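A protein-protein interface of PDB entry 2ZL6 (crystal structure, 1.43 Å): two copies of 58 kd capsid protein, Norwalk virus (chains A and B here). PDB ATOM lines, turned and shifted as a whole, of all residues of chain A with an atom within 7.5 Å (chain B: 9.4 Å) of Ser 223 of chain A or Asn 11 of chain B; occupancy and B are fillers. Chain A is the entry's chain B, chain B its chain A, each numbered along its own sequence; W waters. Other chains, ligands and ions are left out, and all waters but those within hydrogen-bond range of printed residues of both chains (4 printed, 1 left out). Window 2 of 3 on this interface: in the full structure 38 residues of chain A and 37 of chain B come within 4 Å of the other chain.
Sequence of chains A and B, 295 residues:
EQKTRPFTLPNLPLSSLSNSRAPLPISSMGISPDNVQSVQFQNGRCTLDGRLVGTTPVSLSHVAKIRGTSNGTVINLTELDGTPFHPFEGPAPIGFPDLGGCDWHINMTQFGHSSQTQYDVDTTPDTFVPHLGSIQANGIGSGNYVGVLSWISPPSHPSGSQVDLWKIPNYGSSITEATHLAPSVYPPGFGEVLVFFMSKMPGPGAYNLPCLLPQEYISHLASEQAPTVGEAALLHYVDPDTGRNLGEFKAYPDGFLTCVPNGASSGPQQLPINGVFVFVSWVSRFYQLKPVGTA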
ATOM      1  N   CYS A  46      14.749  -6.693   5.509  1.00  0.00           N
ATOM      2  CA  CYS A  46      15.399  -7.575   4.561  1.00  0.00           C
ATOM      3  C   CYS A  46      16.209  -8.588   5.346  1.00  0.00           C
ATOM      4  O   CYS A  46      16.956  -8.224   6.265  1.00  0.00           O
ATOM      5  CB  CYS A  46      16.327  -6.763   3.640  1.00  0.00           C
ATOM      6  SG  CYS A  46      17.109  -7.753   2.334  1.00  0.00           S
ATOM      7  N   ASP A  49      19.911 -13.238   3.788  1.00  0.00           N
ATOM      8  CA  ASP A  49      20.052 -13.913   2.485  1.00  0.00           C
ATOM      9  C   ASP A  49      19.368 -13.154   1.344  1.00  0.00           C
ATOM     10  O   ASP A  49      19.313 -13.656   0.230  1.00  0.00           O
ATOM     11  CB  ASP A  49      19.645 -15.401   2.535  1.00  0.00           C
ATOM     12  CG  ASP A  49      18.144 -15.618   2.671  1.00  0.00           C
ATOM     13  OD1 ASP A  49      17.361 -14.658   2.683  1.00  0.00           O
ATOM     14  OD2 ASP A  49      17.760 -16.791   2.775  1.00  0.00           O
ATOM     15  N   GLY A  50      18.866 -11.957   1.626  1.00  0.00           N
ATOM     16  CA  GLY A  50      18.340 -11.095   0.580  1.00  0.00           C
ATOM     17  C   GLY A  50      16.842 -11.124   0.369  1.00  0.00           C
ATOM     18  O   GLY A  50      16.381 -10.624  -0.641  1.00  0.00           O
ATOM     19  N   VAL A  58      13.523  -2.430  -2.920  1.00  0.00           N
ATOM     20  CA  VAL A  58      14.980  -2.447  -3.141  1.00  0.00           C
ATOM     21  C   VAL A  58      15.579  -1.033  -3.045  1.00  0.00           C
ATOM     22  O   VAL A  58      16.691  -0.848  -2.520  1.00  0.00           O
ATOM     23  CB  VAL A  58      15.273  -3.018  -4.585  1.00  0.00           C
ATOM     24  CG1 VAL A  58      16.700  -2.771  -5.021  1.00  0.00           C
ATOM     25  CG2 VAL A  58      14.922  -4.509  -4.652  1.00  0.00           C
ATOM     26  N   TYR A 217      21.999  -1.077   2.797  1.00  0.00           N
ATOM     27  CA  TYR A 217      22.188  -2.466   3.246  1.00  0.00           C
ATOM     28  C   TYR A 217      21.164  -3.399   2.595  1.00  0.00           C
ATOM     29  O   TYR A 217      21.495  -4.537   2.270  1.00  0.00           O
ATOM     30  CB  TYR A 217      22.051  -2.600   4.769  1.00  0.00           C
ATOM     31  CG  TYR A 217      23.312  -2.274   5.571  1.00  0.00           C
ATOM     32  CD1 TYR A 217      24.125  -1.193   5.248  1.00  0.00           C
ATOM     33  CD2 TYR A 217      23.688  -3.077   6.636  1.00  0.00           C
ATOM     34  CE1 TYR A 217      25.278  -0.901   5.992  1.00  0.00           C
ATOM     35  CE2 TYR A 217      24.822  -2.792   7.381  1.00  0.00           C
ATOM     36  CZ  TYR A 217      25.613  -1.724   7.052  1.00  0.00           C
ATOM     37  OH  TYR A 217      26.749  -1.438   7.801  1.00  0.00           O
ATOM     38  N   ILE A 218      19.944  -2.891   2.459  1.00  0.00           N
ATOM     39  CA  ILE A 218      18.855  -3.651   1.826  1.00  0.00           C
ATOM     40  C   ILE A 218      19.171  -3.958   0.355  1.00  0.00           C
ATOM     41  O   ILE A 218      19.105  -5.121  -0.050  1.00  0.00           O
ATOM     42  CB  ILE A 218      17.536  -2.941   2.014  1.00  0.00           C
ATOM     43  CG1 ILE A 218      17.213  -2.943   3.521  1.00  0.00           C
ATOM     44  CG2 ILE A 218      16.394  -3.644   1.218  1.00  0.00           C
ATOM     45  CD1 ILE A 218      16.149  -2.059   3.904  1.00  0.00           C
ATOM     46  N   SER A 219      19.565  -2.943  -0.419  1.00  0.00           N
ATOM     47  CA  SER A 219      19.906  -3.230  -1.804  1.00  0.00           C
ATOM     48  C   SER A 219      21.133  -4.128  -1.890  1.00  0.00           C
ATOM     49  O   SER A 219      21.189  -5.009  -2.734  1.00  0.00           O
ATOM     50  CB  SER A 219      20.089  -1.960  -2.639  1.00  0.00           C
ATOM     51  OG  SER A 219      20.955  -1.034  -2.010  1.00  0.00           O
ATOM     52  N   HIS A 220      22.112  -3.932  -1.001  1.00  0.00           N
ATOM     53  CA  HIS A 220      23.279  -4.801  -0.982  1.00  0.00           C
ATOM     54  C   HIS A 220      22.916  -6.259  -0.726  1.00  0.00           C
ATOM     55  O   HIS A 220      23.367  -7.148  -1.425  1.00  0.00           O
ATOM     56  CB  HIS A 220      24.285  -4.312   0.083  1.00  0.00           C
ATOM     57  CG  HIS A 220      25.556  -5.100   0.141  1.00  0.00           C
ATOM     58  ND1 HIS A 220      26.725  -4.658  -0.452  1.00  0.00           N
ATOM     59  CD2 HIS A 220      25.866  -6.263   0.764  1.00  0.00           C
ATOM     60  CE1 HIS A 220      27.684  -5.543  -0.232  1.00  0.00           C
ATOM     61  NE2 HIS A 220      27.189  -6.525   0.498  1.00  0.00           N
ATOM     62  N   LEU A 221      22.098  -6.487   0.300  1.00  0.00           N
ATOM     63  CA  LEU A 221      21.736  -7.869   0.659  1.00  0.00           C
ATOM     64  C   LEU A 221      20.846  -8.517  -0.414  1.00  0.00           C
ATOM     65  O   LEU A 221      20.997  -9.718  -0.706  1.00  0.00           O
ATOM     66  CB  LEU A 221      21.022  -7.906   2.020  1.00  0.00           C
ATOM     67  CG  LEU A 221      21.909  -7.573   3.228  1.00  0.00           C
ATOM     68  CD1 LEU A 221      21.034  -7.344   4.473  1.00  0.00           C
ATOM     69  CD2 LEU A 221      22.979  -8.617   3.492  1.00  0.00           C
ATOM     70  N   ALA A 222      19.952  -7.705  -0.993  1.00  0.00           N
ATOM     71  CA  ALA A 222      19.041  -8.184  -2.065  1.00  0.00           C
ATOM     72  C   ALA A 222      19.817  -8.576  -3.315  1.00  0.00           C
ATOM     73  O   ALA A 222      19.419  -9.495  -4.049  1.00  0.00           O
ATOM     74  CB  ALA A 222      17.965  -7.151  -2.386  1.00  0.00           C
ATOM     75  N   SER A 223      20.928  -7.880  -3.553  1.00  0.00           N
ATOM     76  CA  SER A 223      21.825  -8.187  -4.656  1.00  0.00           C
ATOM     77  C   SER A 223      22.691  -9.402  -4.345  1.00  0.00           C
ATOM     78  O   SER A 223      22.852 -10.309  -5.177  1.00  0.00           O
ATOM     79  CB  SER A 223      22.702  -6.967  -4.977  1.00  0.00           C
ATOM     80  OG  SER A 223      23.698  -7.291  -5.935  1.00  0.00           O
ATOM     81  N   GLU A 224      23.284  -9.403  -3.145  1.00  0.00           N
ATOM     82  CA  GLU A 224      24.237 -10.444  -2.758  1.00  0.00           C
ATOM     83  C   GLU A 224      23.602 -11.842  -2.730  1.00  0.00           C
ATOM     84  O   GLU A 224      24.238 -12.827  -3.146  1.00  0.00           O
ATOM     85  CB  GLU A 224      24.865 -10.074  -1.405  1.00  0.00           C
ATOM     86  CG  GLU A 224      25.701 -11.145  -0.735  1.00  0.00           C
ATOM     87  CD  GLU A 224      26.339 -10.662   0.566  1.00  0.00           C
ATOM     88  OE1 GLU A 224      26.004  -9.548   1.049  1.00  0.00           O
ATOM     89  OE2 GLU A 224      27.169 -11.420   1.116  1.00  0.00           O
ATOM     90  N   GLN A 225      22.359 -11.920  -2.245  1.00  0.00           N
ATOM     91  CA  GLN A 225      21.637 -13.202  -2.143  1.00  0.00           C
ATOM     92  C   GLN A 225      22.534 -14.304  -1.536  1.00  0.00           C
ATOM     93  O   GLN A 225      22.696 -15.380  -2.118  1.00  0.00           O
ATOM     94  CB  GLN A 225      21.018 -13.599  -3.504  1.00  0.00           C
ATOM     95  CG  GLN A 225      19.994 -12.584  -4.007  1.00  0.00           C
ATOM     96  CD  GLN A 225      19.649 -12.689  -5.487  1.00  0.00           C
ATOM     97  OE1 GLN A 225      19.763 -13.758  -6.099  1.00  0.00           O
ATOM     98  NE2 GLN A 225      19.223 -11.571  -6.067  1.00  0.00           N
ATOM     99  N   ALA A 226      23.126 -13.999  -0.381  1.00  0.00           N
ATOM    100  CA  ALA A 226      24.082 -14.877   0.308  1.00  0.00           C
ATOM    101  C   ALA A 226      23.619 -16.326   0.330  1.00  0.00           C
ATOM    102  O   ALA A 226      22.526 -16.601   0.841  1.00  0.00           O
ATOM    103  CB  ALA A 226      24.294 -14.387   1.735  1.00  0.00           C
ATOM    104  N   THR B   8      31.896  -7.070  -9.928  1.00  0.00           N
ATOM    105  CA  THR B   8      30.438  -7.200  -9.938  1.00  0.00           C
ATOM    106  C   THR B   8      29.672  -5.888 -10.127  1.00  0.00           C
ATOM    107  O   THR B   8      30.111  -4.817  -9.699  1.00  0.00           O
ATOM    108  CB  THR B   8      29.883  -7.868  -8.652  1.00  0.00           C
ATOM    109  OG1 THR B   8      30.151  -7.021  -7.527  1.00  0.00           O
ATOM    110  CG2 THR B   8      30.505  -9.241  -8.420  1.00  0.00           C
ATOM    111  N   LEU B   9      28.516  -6.003 -10.772  1.00  0.00           N
ATOM    112  CA  LEU B   9      27.464  -4.991 -10.757  1.00  0.00           C
ATOM    113  C   LEU B   9      26.271  -5.545  -9.965  1.00  0.00           C
ATOM    114  O   LEU B   9      26.158  -6.762  -9.798  1.00  0.00           O
ATOM    115  CB  LEU B   9      27.014  -4.657 -12.196  1.00  0.00           C
ATOM    116  CG  LEU B   9      28.094  -3.995 -13.060  1.00  0.00           C
ATOM    117  CD1 LEU B   9      27.588  -3.803 -14.466  1.00  0.00           C
ATOM    118  CD2 LEU B   9      28.511  -2.649 -12.469  1.00  0.00           C
ATOM    119  N   PRO B  10      25.377  -4.671  -9.472  1.00  0.00           N
ATOM    120  CA  PRO B  10      24.227  -5.199  -8.685  1.00  0.00           C
ATOM    121  C   PRO B  10      23.438  -6.257  -9.435  1.00  0.00           C
ATOM    122  O   PRO B  10      23.147  -6.110 -10.636  1.00  0.00           O
ATOM    123  CB  PRO B  10      23.362  -3.969  -8.453  1.00  0.00           C
ATOM    124  CG  PRO B  10      24.393  -2.826  -8.444  1.00  0.00           C
ATOM    125  CD  PRO B  10      25.371  -3.197  -9.529  1.00  0.00           C
ATOM    126  N   ASN B  11      23.149  -7.343  -8.724  1.00  0.00           N
ATOM    127  CA  ASN B  11      22.257  -8.379  -9.251  1.00  0.00           C
ATOM    128  C   ASN B  11      20.812  -8.017  -8.956  1.00  0.00           C
ATOM    129  O   ASN B  11      20.153  -8.671  -8.140  1.00  0.00           O
ATOM    130  CB  ASN B  11      22.632  -9.747  -8.677  1.00  0.00           C
ATOM    131  CG  ASN B  11      21.784 -10.871  -9.253  1.00  0.00           C
ATOM    132  OD1 ASN B  11      21.143 -10.705 -10.292  1.00  0.00           O
ATOM    133  ND2 ASN B  11      21.713 -11.987  -8.527  1.00  0.00           N
ATOM    134  N   LEU B  12      20.344  -6.948  -9.594  1.00  0.00           N
ATOM    135  CA  LEU B  12      19.050  -6.321  -9.342  1.00  0.00           C
ATOM    136  C   LEU B  12      18.486  -5.838 -10.672  1.00  0.00           C
ATOM    137  O   LEU B  12      19.226  -5.256 -11.482  1.00  0.00           O
ATOM    138  CB  LEU B  12      19.235  -5.120  -8.399  1.00  0.00           C
ATOM    139  CG  LEU B  12      19.706  -5.457  -6.973  1.00  0.00           C
ATOM    140  CD1 LEU B  12      20.084  -4.163  -6.226  1.00  0.00           C
ATOM    141  CD2 LEU B  12      18.623  -6.245  -6.201  1.00  0.00           C
ATOM    142  N   PRO B  13      17.188  -6.032 -10.891  1.00  0.00           N
ATOM    143  CA  PRO B  13      16.630  -5.597 -12.184  1.00  0.00           C
ATOM    144  C   PRO B  13      16.616  -4.084 -12.258  1.00  0.00           C
ATOM    145  O   PRO B  13      16.367  -3.405 -11.260  1.00  0.00           O
ATOM    146  CB  PRO B  13      15.194  -6.138 -12.181  1.00  0.00           C
ATOM    147  CG  PRO B  13      14.906  -6.553 -10.768  1.00  0.00           C
ATOM    148  CD  PRO B  13      16.197  -6.658  -9.997  1.00  0.00           C
ATOM    149  N   LEU B  14      16.866  -3.536 -13.444  1.00  0.00           N
ATOM    150  CA  LEU B  14      16.932  -2.064 -13.579  1.00  0.00           C
ATOM    151  C   LEU B  14      15.679  -1.348 -13.102  1.00  0.00           C
ATOM    152  O   LEU B  14      15.748  -0.265 -12.492  1.00  0.00           O
ATOM    153  CB  LEU B  14      17.264  -1.642 -15.022  1.00  0.00           C
ATOM    154  CG  LEU B  14      18.613  -2.145 -15.525  1.00  0.00           C
ATOM    155  CD1 LEU B  14      18.820  -1.720 -16.996  1.00  0.00           C
ATOM    156  CD2 LEU B  14      19.781  -1.637 -14.649  1.00  0.00           C
ATOM    157  N   SER B  16      13.888  -1.886 -10.726  1.00  0.00           N
ATOM    158  CA  SER B  16      13.834  -1.811  -9.262  1.00  0.00           C
ATOM    159  C   SER B  16      14.712  -0.702  -8.690  1.00  0.00           C
ATOM    160  O   SER B  16      14.733  -0.510  -7.486  1.00  0.00           O
ATOM    161  CB  SER B  16      14.268  -3.146  -8.671  1.00  0.00           C
ATOM    162  OG  SER B  16      13.283  -4.128  -8.954  1.00  0.00           O
ATOM    163  N   LEU B  17      15.433  -0.006  -9.568  1.00  0.00           N
ATOM    164  CA  LEU B  17      16.491   0.926  -9.150  1.00  0.00           C
ATOM    165  C   LEU B  17      16.098   2.380  -9.368  1.00  0.00           C
ATOM    166  O   LEU B  17      15.024   2.675  -9.925  1.00  0.00           O
ATOM    167  CB  LEU B  17      17.785   0.582  -9.889  1.00  0.00           C
ATOM    168  CG  LEU B  17      18.232  -0.880  -9.784  1.00  0.00           C
ATOM    169  CD1 LEU B  17      19.561  -1.073 -10.513  1.00  0.00           C
ATOM    170  CD2 LEU B  17      18.352  -1.333  -8.330  1.00  0.00           C
ATOM    171  N   GLU B 216      21.858   2.886  -7.233  1.00  0.00           N
ATOM    172  CA  GLU B 216      22.307   1.669  -6.540  1.00  0.00           C
ATOM    173  C   GLU B 216      23.598   1.085  -7.110  1.00  0.00           C
ATOM    174  O   GLU B 216      24.348   0.374  -6.429  1.00  0.00           O
ATOM    175  CB  GLU B 216      21.198   0.592  -6.492  1.00  0.00           C
ATOM    176  CG  GLU B 216      19.968   1.008  -5.619  1.00  0.00           C
ATOM    177  CD  GLU B 216      19.059   2.066  -6.230  1.00  0.00           C
ATOM    178  OE1 GLU B 216      19.148   2.366  -7.456  1.00  0.00           O
ATOM    179  OE2 GLU B 216      18.201   2.607  -5.481  1.00  0.00           O
ATOM    180  N   TYR B 217      23.858   1.381  -8.394  1.00  0.00           N
ATOM    181  CA  TYR B 217      25.163   1.052  -8.967  1.00  0.00           C
ATOM    182  C   TYR B 217      26.296   1.864  -8.325  1.00  0.00           C
ATOM    183  O   TYR B 217      27.381   1.321  -8.086  1.00  0.00           O
ATOM    184  CB  TYR B 217      25.190   1.284 -10.493  1.00  0.00           C
ATOM    185  CG  TYR B 217      24.596   0.178 -11.336  1.00  0.00           C
ATOM    186  CD1 TYR B 217      23.404  -0.456 -10.979  1.00  0.00           C
ATOM    187  CD2 TYR B 217      25.229  -0.220 -12.496  1.00  0.00           C
ATOM    188  CE1 TYR B 217      22.859  -1.468 -11.781  1.00  0.00           C
ATOM    189  CE2 TYR B 217      24.686  -1.210 -13.313  1.00  0.00           C
ATOM    190  CZ  TYR B 217      23.518  -1.832 -12.933  1.00  0.00           C
ATOM    191  OH  TYR B 217      23.008  -2.844 -13.742  1.00  0.00           O
ATOM    192  N   HIS B 220      26.961   0.525  -4.891  1.00  0.00           N
ATOM    193  CA  HIS B 220      27.626  -0.772  -5.070  1.00  0.00           C
ATOM    194  C   HIS B 220      29.113  -0.618  -5.426  1.00  0.00           C
ATOM    195  O   HIS B 220      29.991  -1.261  -4.839  1.00  0.00           O
ATOM    196  CB  HIS B 220      26.909  -1.576  -6.162  1.00  0.00           C
ATOM    197  CG  HIS B 220      27.412  -2.973  -6.310  1.00  0.00           C
ATOM    198  ND1 HIS B 220      28.497  -3.323  -7.089  1.00  0.00           N
ATOM    199  CD2 HIS B 220      26.921  -4.133  -5.809  1.00  0.00           C
ATOM    200  CE1 HIS B 220      28.680  -4.632  -7.018  1.00  0.00           C
ATOM    201  NE2 HIS B 220      27.728  -5.146  -6.260  1.00  0.00           N
ATOM    202  N   GLU B 224      32.342  -1.650  -3.286  1.00  0.00           N
ATOM    203  CA  GLU B 224      33.154  -2.718  -3.839  1.00  0.00           C
ATOM    204  C   GLU B 224      34.648  -2.334  -3.964  1.00  0.00           C
ATOM    205  O   GLU B 224      35.540  -3.164  -3.761  1.00  0.00           O
ATOM    206  CB  GLU B 224      32.570  -3.110  -5.207  1.00  0.00           C
ATOM    207  CG  GLU B 224      33.427  -4.108  -6.033  1.00  0.00           C
ATOM    208  CD  GLU B 224      32.789  -4.520  -7.359  1.00  0.00           C
ATOM    209  OE1 GLU B 224      31.730  -3.944  -7.723  1.00  0.00           O
ATOM    210  OE2 GLU B 224      33.355  -5.407  -8.043  1.00  0.00           O
ATOM    211  N   HIS B 236      26.686  -8.649 -20.146  1.00  0.00           N
ATOM    212  CA  HIS B 236      25.445  -9.062 -20.782  1.00  0.00           C
ATOM    213  C   HIS B 236      24.271  -8.455 -20.042  1.00  0.00           C
ATOM    214  O   HIS B 236      24.288  -8.399 -18.795  1.00  0.00           O
ATOM    215  CB  HIS B 236      25.297 -10.589 -20.769  1.00  0.00           C
ATOM    216  CG  HIS B 236      26.277 -11.300 -21.653  1.00  0.00           C
ATOM    217  ND1 HIS B 236      26.457 -12.667 -21.614  1.00  0.00           N
ATOM    218  CD2 HIS B 236      27.144 -10.832 -22.585  1.00  0.00           C
ATOM    219  CE1 HIS B 236      27.383 -13.012 -22.494  1.00  0.00           C
ATOM    220  NE2 HIS B 236      27.817 -11.918 -23.096  1.00  0.00           N
ATOM    221  N   VAL B 238      20.710  -9.348 -19.048  1.00  0.00           N
ATOM    222  CA  VAL B 238      20.154 -10.702 -18.926  1.00  0.00           C
ATOM    223  C   VAL B 238      18.721 -10.641 -18.415  1.00  0.00           C
ATOM    224  O   VAL B 238      18.417  -9.896 -17.479  1.00  0.00           O
ATOM    225  CB  VAL B 238      21.027 -11.569 -17.978  1.00  0.00           C
ATOM    226  CG1 VAL B 238      20.423 -12.952 -17.760  1.00  0.00           C
ATOM    227  CG2 VAL B 238      22.451 -11.708 -18.518  1.00  0.00           C
ATOM    228  N   ASP B 239      17.832 -11.429 -19.019  1.00  0.00           N
ATOM    229  CA  ASP B 239      16.548 -11.715 -18.392  1.00  0.00           C
ATOM    230  C   ASP B 239      16.769 -12.752 -17.285  1.00  0.00           C
ATOM    231  O   ASP B 239      17.245 -13.852 -17.552  1.00  0.00           O
ATOM    232  CB  ASP B 239      15.534 -12.235 -19.417  1.00  0.00           C
ATOM    233  CG  ASP B 239      14.225 -12.642 -18.767  1.00  0.00           C
ATOM    234  OD1 ASP B 239      13.483 -11.753 -18.321  1.00  0.00           O
ATOM    235  OD2 ASP B 239      13.950 -13.862 -18.678  1.00  0.00           O
ATOM    236  N   PRO B 240      16.460 -12.393 -16.024  1.00  0.00           N
ATOM    237  CA  PRO B 240      16.763 -13.268 -14.876  1.00  0.00           C
ATOM    238  C   PRO B 240      16.120 -14.674 -14.887  1.00  0.00           C
ATOM    239  O   PRO B 240      16.807 -15.679 -14.623  1.00  0.00           O
ATOM    240  CB  PRO B 240      16.245 -12.462 -13.674  1.00  0.00           C
ATOM    241  CG  PRO B 240      16.140 -11.077 -14.139  1.00  0.00           C
ATOM    242  CD  PRO B 240      15.844 -11.122 -15.602  1.00  0.00           C
ATOM    243  N   ASP B 241      14.824 -14.727 -15.175  1.00  0.00           N
ATOM    244  CA  ASP B 241      14.055 -15.985 -15.157  1.00  0.00           C
ATOM    245  C   ASP B 241      14.546 -16.994 -16.188  1.00  0.00           C
ATOM    246  O   ASP B 241      14.797 -18.175 -15.883  1.00  0.00           O
ATOM    247  CB  ASP B 241      12.582 -15.685 -15.426  1.00  0.00           C
ATOM    248  CG  ASP B 241      11.969 -14.813 -14.350  1.00  0.00           C
ATOM    249  OD1 ASP B 241      12.098 -15.178 -13.160  1.00  0.00           O
ATOM    250  OD2 ASP B 241      11.378 -13.760 -14.692  1.00  0.00           O
ATOM    251  N   ASN B 274      13.318  -4.819 -17.110  1.00  0.00           N
ATOM    252  CA  ASN B 274      13.389  -5.690 -15.947  1.00  0.00           C
ATOM    253  C   ASN B 274      14.598  -6.626 -15.973  1.00  0.00           C
ATOM    254  O   ASN B 274      14.637  -7.609 -15.231  1.00  0.00           O
ATOM    255  CB  ASN B 274      12.077  -6.474 -15.773  1.00  0.00           C
ATOM    256  CG  ASN B 274      11.862  -7.501 -16.871  1.00  0.00           C
ATOM    257  OD1 ASN B 274      12.469  -7.433 -17.952  1.00  0.00           O
ATOM    258  ND2 ASN B 274      11.012  -8.491 -16.586  1.00  0.00           N
ATOM    259  N   GLY B 275      15.597  -6.338 -16.820  1.00  0.00           N
ATOM    260  CA  GLY B 275      16.788  -7.164 -16.885  1.00  0.00           C
ATOM    261  C   GLY B 275      17.887  -6.734 -15.914  1.00  0.00           C
ATOM    262  O   GLY B 275      17.748  -5.723 -15.222  1.00  0.00           O
ATOM    263  N   VAL B 276      18.961  -7.508 -15.902  1.00  0.00           N
ATOM    264  CA  VAL B 276      20.098  -7.354 -14.972  1.00  0.00           C
ATOM    265  C   VAL B 276      21.372  -7.300 -15.777  1.00  0.00           C
ATOM    266  O   VAL B 276      21.594  -8.169 -16.630  1.00  0.00           O
ATOM    267  CB  VAL B 276      20.136  -8.574 -13.975  1.00  0.00           C
ATOM    268  CG1 VAL B 276      21.366  -8.576 -13.091  1.00  0.00           C
ATOM    269  CG2 VAL B 276      18.848  -8.616 -13.132  1.00  0.00           C
ATOM    270  N   PHE B 277      22.212  -6.293 -15.545  1.00  0.00           N
ATOM    271  CA  PHE B 277      23.564  -6.324 -16.113  1.00  0.00           C
ATOM    272  C   PHE B 277      24.496  -7.235 -15.354  1.00  0.00           C
ATOM    273  O   PHE B 277      24.583  -7.170 -14.118  1.00  0.00           O
ATOM    274  CB  PHE B 277      24.182  -4.928 -16.179  1.00  0.00           C
ATOM    275  CG  PHE B 277      23.649  -4.107 -17.295  1.00  0.00           C
ATOM    276  CD1 PHE B 277      23.930  -4.479 -18.611  1.00  0.00           C
ATOM    277  CD2 PHE B 277      22.851  -2.995 -17.059  1.00  0.00           C
ATOM    278  CE1 PHE B 277      23.470  -3.716 -19.654  1.00  0.00           C
ATOM    279  CE2 PHE B 277      22.359  -2.235 -18.099  1.00  0.00           C
ATOM    280  CZ  PHE B 277      22.661  -2.618 -19.421  1.00  0.00           C
ATOM    281  N   VAL B 278      25.177  -8.106 -16.083  1.00  0.00           N
ATOM    282  CA  VAL B 278      26.057  -9.078 -15.486  1.00  0.00           C
ATOM    283  C   VAL B 278      27.430  -8.930 -16.096  1.00  0.00           C
ATOM    284  O   VAL B 278      27.569  -8.944 -17.318  1.00  0.00           O
ATOM    285  CB  VAL B 278      25.544 -10.541 -15.719  1.00  0.00           C
ATOM    286  CG1 VAL B 278      26.459 -11.547 -15.068  1.00  0.00           C
ATOM    287  CG2 VAL B 278      24.116 -10.704 -15.234  1.00  0.00           C
ATOM    288  N   PHE B 279      28.439  -8.802 -15.244  1.00  0.00           N
ATOM    289  CA  PHE B 279      29.812  -8.727 -15.707  1.00  0.00           C
ATOM    290  C   PHE B 279      30.227 -10.070 -16.302  1.00  0.00           C
ATOM    291  O   PHE B 279      30.032 -11.121 -15.669  1.00  0.00           O
ATOM    292  CB  PHE B 279      30.733  -8.365 -14.542  1.00  0.00           C
ATOM    293  CG  PHE B 279      32.198  -8.479 -14.870  1.00  0.00           C
ATOM    294  CD1 PHE B 279      32.835  -7.485 -15.607  1.00  0.00           C
ATOM    295  CD2 PHE B 279      32.935  -9.585 -14.446  1.00  0.00           C
ATOM    296  CE1 PHE B 279      34.189  -7.581 -15.911  1.00  0.00           C
ATOM    297  CE2 PHE B 279      34.305  -9.698 -14.743  1.00  0.00           C
ATOM    298  CZ  PHE B 279      34.930  -8.674 -15.467  1.00  0.00           C
HETATM  299  O   HOH W   1      17.580  -9.718  -8.164  1.00  0.00           O
HETATM  300  O   HOH W   2      12.774  -0.587  -5.536  1.00  0.00           O
HETATM  301  O   HOH W   3      23.863 -12.444  -6.476  1.00  0.00           O
HETATM  302  O   HOH W   4      19.823 -14.173  -8.562  1.00  0.00           O
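Positions printed for both chains: 217, 220 and 224.
The backbone carbonyl oxygen (O) of Ala 222 of chain A sits at hydrogen-bond distance from the side-chain amide nitrogen (NE2) of Gln 225 of chain A, at 2.9 Å.
Water W4 lies within hydrogen-bond range of OE1 of Gln 225 of chain A (2.5 Å) and ND2 of Asn 11 of chain B (2.9 Å). Water W3 lies within hydrogen-bond range of O of Ser 223 of chain A (2.7 Å), ND2 of Asn 11 of chain B (3.0 Å) and O of Glu 224 of chain A (3.4 Å). Water W2 lies within hydrogen-bond range of O of Ser 16 of chain B (2.8 Å) and N of Val 58 of chain A (3.3 Å). Water W1 bridges O of Asn 11 of chain B (2.8 Å) and NE2 of Gln 225 of chain A (3.2 Å).
Among the printed residues, pairs that only touch across the chains: Val 58 of chain A with Leu 12 of chain B (3.9 Å), Val 58 of chain A with Ser 16 of chain B (3.9 Å), Val 58 of chain A with Leu 17 of chain B (3.97 Å), Ser 219 of chain A with Leu 12 of chain B (3.8 Å), Ala 222 of chain A with Leu 12 of chain B (3.9 Å), Ser 223 of chain A with Pro 10 of chain B (3.5 Å), Ser 223 of chain A with Leu 12 of chain B (3.9 Å) and Gln 225 of chain A with Asn 11 of chain B (3.5 Å).
Of the printed residues of chain B, Ser 219 of chain A touches Leu 12 (3.8 Å). Ser 223 of chain A touches just these residues of chain B: Pro 10 (3.5 Å), Asn 11 (2.8 Å) and Leu 12 (3.9 Å). Printed residues of chain B within 4 Å of Gln 225 of chain A: Asn 11. Of chain A, only Ser 223 (2.8 Å) and Gln 225 (3.5 Å) come within 4 Å of Asn 11 of chain B. Of the printed residues of chain A, Ser 16 of chain B touches Val 58 (3.9 Å). Of the printed residues of chain A, Leu 17 of chain B touches Val 58. Val 238 of chain B touches none of the printed residues of chain A. Pro 240 of chain B touches none of the printed residues of chain A. The nearest residue of chain A that does not touch Asn 11 of chain B is Ala 222 of chain A (4.2 Å).
Hydrophobic or aromatic side chains of chain B that line the printed part of chain A: Leu 12 and Leu 17. Of the 14 printed residues of chain A, 5 touch a printed residue of chain B. Printed residues of chain A that touch a printed residue of chain B: Val 58, Ser 219, Ala 222, Ser 223 and Gln 225. Hydrophobic or aromatic side chains of chain A that line the printed part of chain B: Val 58 and Ala 222.
The backbone NH of Asn 11 of chain B lies within hydrogen-bond range of the side-chain hydroxyl of Ser 223 of chain A (2.8 Å).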
